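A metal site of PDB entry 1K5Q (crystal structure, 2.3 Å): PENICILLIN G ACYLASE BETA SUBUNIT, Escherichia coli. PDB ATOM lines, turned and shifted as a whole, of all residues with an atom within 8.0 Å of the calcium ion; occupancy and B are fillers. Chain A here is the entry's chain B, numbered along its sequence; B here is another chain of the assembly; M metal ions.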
ATOM      1  N   GLY A  72      -0.032  10.869  18.452  1.00  0.00           N
ATOM      2  CA  GLY A  72       0.540   9.785  19.229  1.00  0.00           C
ATOM      3  C   GLY A  72      -0.024   8.515  18.603  1.00  0.00           C
ATOM      4  O   GLY A  72      -0.878   8.602  17.726  1.00  0.00           O
ATOM      5  N   ASP A  73       0.467   7.345  19.020  1.00  0.00           N
ATOM      6  CA  ASP A  73      -0.036   6.090  18.492  1.00  0.00           C
ATOM      7  C   ASP A  73      -1.061   5.522  19.458  1.00  0.00           C
ATOM      8  O   ASP A  73      -0.701   4.845  20.437  1.00  0.00           O
ATOM      9  CB  ASP A  73       1.088   5.068  18.295  1.00  0.00           C
ATOM     10  CG  ASP A  73       0.618   3.799  17.602  1.00  0.00           C
ATOM     11  OD1 ASP A  73      -0.609   3.608  17.421  1.00  0.00           O
ATOM     12  OD2 ASP A  73       1.418   2.903  17.208  1.00  0.00           O
ATOM     13  N   ASP A  74      -2.325   5.809  19.185  1.00  0.00           N
ATOM     14  CA  ASP A  74      -3.410   5.316  20.023  1.00  0.00           C
ATOM     15  C   ASP A  74      -4.268   4.321  19.250  1.00  0.00           C
ATOM     16  O   ASP A  74      -5.384   4.030  19.651  1.00  0.00           O
ATOM     17  CB  ASP A  74      -4.274   6.465  20.527  1.00  0.00           C
ATOM     18  CG  ASP A  74      -4.918   7.261  19.405  1.00  0.00           C
ATOM     19  OD1 ASP A  74      -4.687   6.920  18.227  1.00  0.00           O
ATOM     20  OD2 ASP A  74      -5.654   8.258  19.645  1.00  0.00           O
ATOM     21  N   VAL A  75      -3.725   3.787  18.152  1.00  0.00           N
ATOM     22  CA  VAL A  75      -4.462   2.832  17.337  1.00  0.00           C
ATOM     23  C   VAL A  75      -3.614   1.665  16.851  1.00  0.00           C
ATOM     24  O   VAL A  75      -2.595   1.861  16.195  1.00  0.00           O
ATOM     25  CB  VAL A  75      -5.038   3.503  16.091  1.00  0.00           C
ATOM     26  CG1 VAL A  75      -5.849   2.505  15.279  1.00  0.00           C
ATOM     27  CG2 VAL A  75      -5.888   4.717  16.473  1.00  0.00           C
ATOM     28  N   ASP A  76      -4.047   0.451  17.184  1.00  0.00           N
ATOM     29  CA  ASP A  76      -3.371  -0.745  16.752  1.00  0.00           C
ATOM     30  C   ASP A  76      -4.358  -1.616  15.947  1.00  0.00           C
ATOM     31  O   ASP A  76      -5.566  -1.521  16.089  1.00  0.00           O
ATOM     32  CB  ASP A  76      -2.841  -1.528  17.959  1.00  0.00           C
ATOM     33  CG  ASP A  76      -1.776  -0.779  18.713  1.00  0.00           C
ATOM     34  OD1 ASP A  76      -1.092   0.105  18.106  1.00  0.00           O
ATOM     35  OD2 ASP A  76      -1.566  -1.031  19.940  1.00  0.00           O
ATOM     36  N   ILE A  77      -3.820  -2.492  15.123  1.00  0.00           N
ATOM     37  CA  ILE A  77      -4.671  -3.337  14.301  1.00  0.00           C
ATOM     38  C   ILE A  77      -4.507  -4.779  14.731  1.00  0.00           C
ATOM     39  O   ILE A  77      -3.374  -5.281  14.871  1.00  0.00           O
ATOM     40  CB  ILE A  77      -4.335  -3.160  12.830  1.00  0.00           C
ATOM     41  CG1 ILE A  77      -4.857  -1.810  12.346  1.00  0.00           C
ATOM     42  CG2 ILE A  77      -4.942  -4.271  12.009  1.00  0.00           C
ATOM     43  CD1 ILE A  77      -4.642  -1.580  10.886  1.00  0.00           C
ATOM     44  N   SER A 140      -8.308  -1.118  16.372  1.00  0.00           N
ATOM     45  CA  SER A 140      -8.500  -0.885  17.789  1.00  0.00           C
ATOM     46  C   SER A 140      -8.035   0.491  18.269  1.00  0.00           C
ATOM     47  O   SER A 140      -6.844   0.784  18.230  1.00  0.00           O
ATOM     48  CB  SER A 140      -7.740  -1.939  18.562  1.00  0.00           C
ATOM     49  OG  SER A 140      -8.158  -1.919  19.905  1.00  0.00           O
ATOM     50  N   PRO A 197      -2.650   2.831  24.906  1.00  0.00           N
ATOM     51  CA  PRO A 197      -2.660   1.444  25.345  1.00  0.00           C
ATOM     52  C   PRO A 197      -1.409   0.995  26.082  1.00  0.00           C
ATOM     53  O   PRO A 197      -0.269   1.396  25.796  1.00  0.00           O
ATOM     54  CB  PRO A 197      -2.795   0.665  24.033  1.00  0.00           C
ATOM     55  CG  PRO A 197      -2.127   1.549  23.054  1.00  0.00           C
ATOM     56  CD  PRO A 197      -2.553   2.919  23.443  1.00  0.00           C
ATOM     57  N   ARG A 199       0.610  -1.799  26.199  1.00  0.00           N
ATOM     58  CA  ARG A 199       0.850  -2.934  25.314  1.00  0.00           C
ATOM     59  C   ARG A 199       1.674  -4.030  25.962  1.00  0.00           C
ATOM     60  O   ARG A 199       2.467  -3.768  26.867  1.00  0.00           O
ATOM     61  CB  ARG A 199       1.557  -2.454  24.058  1.00  0.00           C
ATOM     62  CG  ARG A 199       0.755  -1.419  23.257  1.00  0.00           C
ATOM     63  CD  ARG A 199       1.480  -1.002  21.973  1.00  0.00           C
ATOM     64  NE  ARG A 199       0.720  -0.161  21.058  1.00  0.00           N
ATOM     65  CZ  ARG A 199       0.683   1.176  21.071  1.00  0.00           C
ATOM     66  NH1 ARG A 199       1.294   1.886  21.996  1.00  0.00           N
ATOM     67  NH2 ARG A 199      -0.008   1.800  20.146  1.00  0.00           N
ATOM     68  N   HIS A 203       5.445  -6.037  22.004  1.00  0.00           N
ATOM     69  CA  HIS A 203       4.494  -5.541  21.020  1.00  0.00           C
ATOM     70  C   HIS A 203       5.082  -4.343  20.273  1.00  0.00           C
ATOM     71  O   HIS A 203       5.389  -3.319  20.853  1.00  0.00           O
ATOM     72  CB  HIS A 203       3.201  -5.140  21.746  1.00  0.00           C
ATOM     73  CG  HIS A 203       2.105  -4.629  20.863  1.00  0.00           C
ATOM     74  ND1 HIS A 203       0.784  -4.637  21.259  1.00  0.00           N
ATOM     75  CD2 HIS A 203       2.117  -4.090  19.623  1.00  0.00           C
ATOM     76  CE1 HIS A 203       0.036  -4.117  20.299  1.00  0.00           C
ATOM     77  NE2 HIS A 203       0.822  -3.791  19.285  1.00  0.00           N
ATOM     78  N   ASP A 204       5.252  -4.485  18.974  1.00  0.00           N
ATOM     79  CA  ASP A 204       5.759  -3.395  18.153  1.00  0.00           C
ATOM     80  C   ASP A 204       4.561  -2.629  17.637  1.00  0.00           C
ATOM     81  O   ASP A 204       3.868  -3.135  16.763  1.00  0.00           O
ATOM     82  CB  ASP A 204       6.543  -3.963  16.964  1.00  0.00           C
ATOM     83  CG  ASP A 204       7.277  -2.904  16.191  1.00  0.00           C
ATOM     84  OD1 ASP A 204       6.689  -1.843  15.901  1.00  0.00           O
ATOM     85  OD2 ASP A 204       8.460  -3.078  15.817  1.00  0.00           O
ATOM     86  N   PRO A 205       4.306  -1.433  18.154  1.00  0.00           N
ATOM     87  CA  PRO A 205       3.095  -0.673  17.857  1.00  0.00           C
ATOM     88  C   PRO A 205       3.023  -0.156  16.408  1.00  0.00           C
ATOM     89  O   PRO A 205       2.061   0.468  16.017  1.00  0.00           O
ATOM     90  CB  PRO A 205       3.183   0.484  18.848  1.00  0.00           C
ATOM     91  CG  PRO A 205       4.634   0.693  18.965  1.00  0.00           C
ATOM     92  CD  PRO A 205       5.185  -0.689  19.062  1.00  0.00           C
ATOM     93  N   ARG A 206       4.033  -0.448  15.619  1.00  0.00           N
ATOM     94  CA  ARG A 206       4.049  -0.029  14.237  1.00  0.00           C
ATOM     95  C   ARG A 206       3.508  -1.118  13.327  1.00  0.00           C
ATOM     96  O   ARG A 206       3.288  -0.883  12.160  1.00  0.00           O
ATOM     97  CB  ARG A 206       5.474   0.292  13.822  1.00  0.00           C
ATOM     98  CG  ARG A 206       6.193   1.281  14.700  1.00  0.00           C
ATOM     99  CD  ARG A 206       7.634   1.382  14.336  1.00  0.00           C
ATOM    100  NE  ARG A 206       8.280   0.098  14.513  1.00  0.00           N
ATOM    101  CZ  ARG A 206       9.557  -0.122  14.330  1.00  0.00           C
ATOM    102  NH1 ARG A 206      10.354   0.858  13.945  1.00  0.00           N
ATOM    103  NH2 ARG A 206      10.042  -1.344  14.538  1.00  0.00           N
ATOM    104  N   LEU A 207       3.292  -2.311  13.867  1.00  0.00           N
ATOM    105  CA  LEU A 207       2.827  -3.451  13.078  1.00  0.00           C
ATOM    106  C   LEU A 207       1.635  -4.170  13.715  1.00  0.00           C
ATOM    107  O   LEU A 207       1.429  -4.115  14.927  1.00  0.00           O
ATOM    108  CB  LEU A 207       3.990  -4.412  12.869  1.00  0.00           C
ATOM    109  CG  LEU A 207       5.168  -3.675  12.228  1.00  0.00           C
ATOM    110  CD1 LEU A 207       6.452  -4.467  12.328  1.00  0.00           C
ATOM    111  CD2 LEU A 207       4.897  -3.346  10.789  1.00  0.00           C
ATOM    112  N   PRO A 208       0.825  -4.835  12.907  1.00  0.00           N
ATOM    113  CA  PRO A 208      -0.358  -5.519  13.415  1.00  0.00           C
ATOM    114  C   PRO A 208      -0.044  -6.606  14.422  1.00  0.00           C
ATOM    115  O   PRO A 208       1.075  -7.096  14.464  1.00  0.00           O
ATOM    116  CB  PRO A 208      -0.985  -6.102  12.148  1.00  0.00           C
ATOM    117  CG  PRO A 208      -0.501  -5.239  11.060  1.00  0.00           C
ATOM    118  CD  PRO A 208       0.916  -4.936  11.443  1.00  0.00           C
ATOM    119  N   TRP A 217      -4.338  -5.670  24.564  1.00  0.00           N
ATOM    120  CA  TRP A 217      -3.792  -4.649  25.416  1.00  0.00           C
ATOM    121  C   TRP A 217      -4.055  -5.018  26.862  1.00  0.00           C
ATOM    122  O   TRP A 217      -5.071  -5.628  27.182  1.00  0.00           O
ATOM    123  CB  TRP A 217      -4.444  -3.304  25.119  1.00  0.00           C
ATOM    124  CG  TRP A 217      -4.153  -2.745  23.764  1.00  0.00           C
ATOM    125  CD1 TRP A 217      -3.114  -3.048  22.947  1.00  0.00           C
ATOM    126  CD2 TRP A 217      -4.911  -1.748  23.092  1.00  0.00           C
ATOM    127  NE1 TRP A 217      -3.182  -2.285  21.804  1.00  0.00           N
ATOM    128  CE2 TRP A 217      -4.290  -1.498  21.870  1.00  0.00           C
ATOM    129  CE3 TRP A 217      -6.085  -1.053  23.398  1.00  0.00           C
ATOM    130  CZ2 TRP A 217      -4.770  -0.564  20.960  1.00  0.00           C
ATOM    131  CZ3 TRP A 217      -6.558  -0.144  22.502  1.00  0.00           C
ATOM    132  CH2 TRP A 217      -5.912   0.086  21.292  1.00  0.00           C
ATOM    133  N   ALA A 250       5.753   8.242  18.048  1.00  0.00           N
ATOM    134  CA  ALA A 250       4.765   8.864  17.204  1.00  0.00           C
ATOM    135  C   ALA A 250       3.765   7.881  16.624  1.00  0.00           C
ATOM    136  O   ALA A 250       3.911   6.662  16.744  1.00  0.00           O
ATOM    137  CB  ALA A 250       5.436   9.569  16.068  1.00  0.00           C
ATOM    138  N   SER A 251       2.769   8.453  15.967  1.00  0.00           N
ATOM    139  CA  SER A 251       1.773   7.717  15.205  1.00  0.00           C
ATOM    140  C   SER A 251       2.492   6.706  14.320  1.00  0.00           C
ATOM    141  O   SER A 251       3.606   6.953  13.846  1.00  0.00           O
ATOM    142  CB  SER A 251       1.013   8.710  14.345  1.00  0.00           C
ATOM    143  OG  SER A 251       0.132   8.044  13.455  1.00  0.00           O
ATOM    144  N   ASP A 252       1.854   5.561  14.099  1.00  0.00           N
ATOM    145  CA  ASP A 252       2.439   4.521  13.251  1.00  0.00           C
ATOM    146  C   ASP A 252       2.356   4.787  11.756  1.00  0.00           C
ATOM    147  O   ASP A 252       2.904   4.004  10.984  1.00  0.00           O
ATOM    148  CB  ASP A 252       1.889   3.117  13.601  1.00  0.00           C
ATOM    149  CG  ASP A 252       0.415   2.977  13.327  1.00  0.00           C
ATOM    150  OD1 ASP A 252      -0.040   3.390  12.261  1.00  0.00           O
ATOM    151  OD2 ASP A 252      -0.355   2.416  14.127  1.00  0.00           O
ATOM    152  N   LEU A 253       1.725   5.876  11.334  1.00  0.00           N
ATOM    153  CA  LEU A 253       1.619   6.204   9.909  1.00  0.00           C
ATOM    154  C   LEU A 253       2.989   6.223   9.257  1.00  0.00           C
ATOM    155  O   LEU A 253       3.877   6.909   9.745  1.00  0.00           O
ATOM    156  CB  LEU A 253       0.972   7.582   9.692  1.00  0.00           C
ATOM    157  CG  LEU A 253      -0.473   7.783  10.137  1.00  0.00           C
ATOM    158  CD1 LEU A 253      -0.896   9.262  10.061  1.00  0.00           C
ATOM    159  CD2 LEU A 253      -1.358   6.924   9.265  1.00  0.00           C
ATOM    160  N   SER B 150      -5.724   7.391  13.185  1.00  0.00           N
ATOM    161  CA  SER B 150      -4.699   7.198  12.177  1.00  0.00           C
ATOM    162  C   SER B 150      -3.860   5.937  12.379  1.00  0.00           C
ATOM    163  O   SER B 150      -3.258   5.732  13.448  1.00  0.00           O
ATOM    164  CB  SER B 150      -3.754   8.400  12.151  1.00  0.00           C
ATOM    165  OG  SER B 150      -4.442   9.606  11.849  1.00  0.00           O
ATOM    166  N   THR B 151      -3.797   5.113  11.356  1.00  0.00           N
ATOM    167  CA  THR B 151      -2.934   3.949  11.400  1.00  0.00           C
ATOM    168  C   THR B 151      -2.685   3.425  10.009  1.00  0.00           C
ATOM    169  O   THR B 151      -3.548   3.509   9.134  1.00  0.00           O
ATOM    170  CB  THR B 151      -3.551   2.865  12.251  1.00  0.00           C
ATOM    171  OG1 THR B 151      -2.533   1.929  12.633  1.00  0.00           O
ATOM    172  CG2 THR B 151      -4.586   2.046  11.466  1.00  0.00           C
ATOM    173  N   SER B 152      -1.500   2.852   9.803  1.00  0.00           N
ATOM    174  CA  SER B 152      -1.121   2.255   8.530  1.00  0.00           C
ATOM    175  C   SER B 152      -0.324   0.984   8.788  1.00  0.00           C
ATOM    176  O   SER B 152       0.516   0.596   7.985  1.00  0.00           O
ATOM    177  CB  SER B 152      -0.269   3.250   7.712  1.00  0.00           C
ATOM    178  OG  SER B 152       1.031   3.424   8.283  1.00  0.00           O
ATOM    179  N   GLU B 153      -0.613   0.309   9.908  1.00  0.00           N
ATOM    180  CA  GLU B 153       0.109  -0.906  10.306  1.00  0.00           C
ATOM    181  C   GLU B 153       0.120  -1.978   9.245  1.00  0.00           C
ATOM    182  O   GLU B 153       1.121  -2.670   9.115  1.00  0.00           O
ATOM    183  CB  GLU B 153      -0.444  -1.477  11.598  1.00  0.00           C
ATOM    184  CG  GLU B 153      -0.070  -0.668  12.815  1.00  0.00           C
ATOM    185  CD  GLU B 153      -0.613  -1.245  14.093  1.00  0.00           C
ATOM    186  OE1 GLU B 153      -1.103  -2.396  14.065  1.00  0.00           O
ATOM    187  OE2 GLU B 153      -0.538  -0.549  15.126  1.00  0.00           O
ATOM    188  N   ASN B 156       2.456  -0.854   6.804  1.00  0.00           N
ATOM    189  CA  ASN B 156       3.748  -0.928   7.444  1.00  0.00           C
ATOM    190  C   ASN B 156       4.355  -2.311   7.334  1.00  0.00           C
ATOM    191  O   ASN B 156       5.520  -2.430   6.975  1.00  0.00           O
ATOM    192  CB  ASN B 156       3.662  -0.513   8.906  1.00  0.00           C
ATOM    193  CG  ASN B 156       3.351   0.963   9.071  1.00  0.00           C
ATOM    194  OD1 ASN B 156       3.307   1.724   8.111  1.00  0.00           O
ATOM    195  ND2 ASN B 156       3.115   1.379  10.320  1.00  0.00           N
HETATM  196 CA    CA M   1      -0.232   1.288  16.155  1.00  0.00          CA
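OE1 of Glu 153 of chain B sits at hydrogen-bond distance from N of Ile 77. The side-chain carboxylate (OD2) of Asp 76 is in salt-bridge range of the guanidinium group (NE) of Arg 199, at 2.7 Å. NH2 of Arg 199 lies within hydrogen-bond range of O of Asp 73. The backbone carbonyl oxygen (O) of Asp 252 sits at hydrogen-bond distance from the side-chain amide nitrogen (ND2) of Asn 156 of chain B (2.7 Å). NE1 of Trp 217 is in hydrogen-bond range of OD2 of Asp 76 (2.8 Å). The side-chain carboxylate of Asp 252 lies within hydrogen-bond range of the backbone NH of Ser 152 of chain B, 2.9 Å away. O of Asp 76 lies within hydrogen-bond range of N of Ser 140 (2.8 Å). OD1 of Asp 252 lies within hydrogen-bond range of OG1 of Thr 151 of chain B (2.9 Å).
Within 4 Å of the calcium ion: Asp 73, Val 75, Asp 76, Pro 205, Asp 252 and Glu 153 of chain B.
The calcium ion is bound by OE2 of Glu 153 of chain B. OD2 of Asp 252 is bound to the calcium ion, 2.3 Å away. The calcium ion is bound by O of Val 75, 2.4 Å away. The calcium ion is bound by OD1 of Asp 76 (2.4 Å). The calcium ion is bound by O of Pro 205, at 2.4 Å. OD2 of Asp 73 binds the calcium ion (2.5 Å). OD1 of Asp 73 is bound to the calcium ion, at 2.7 Å.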
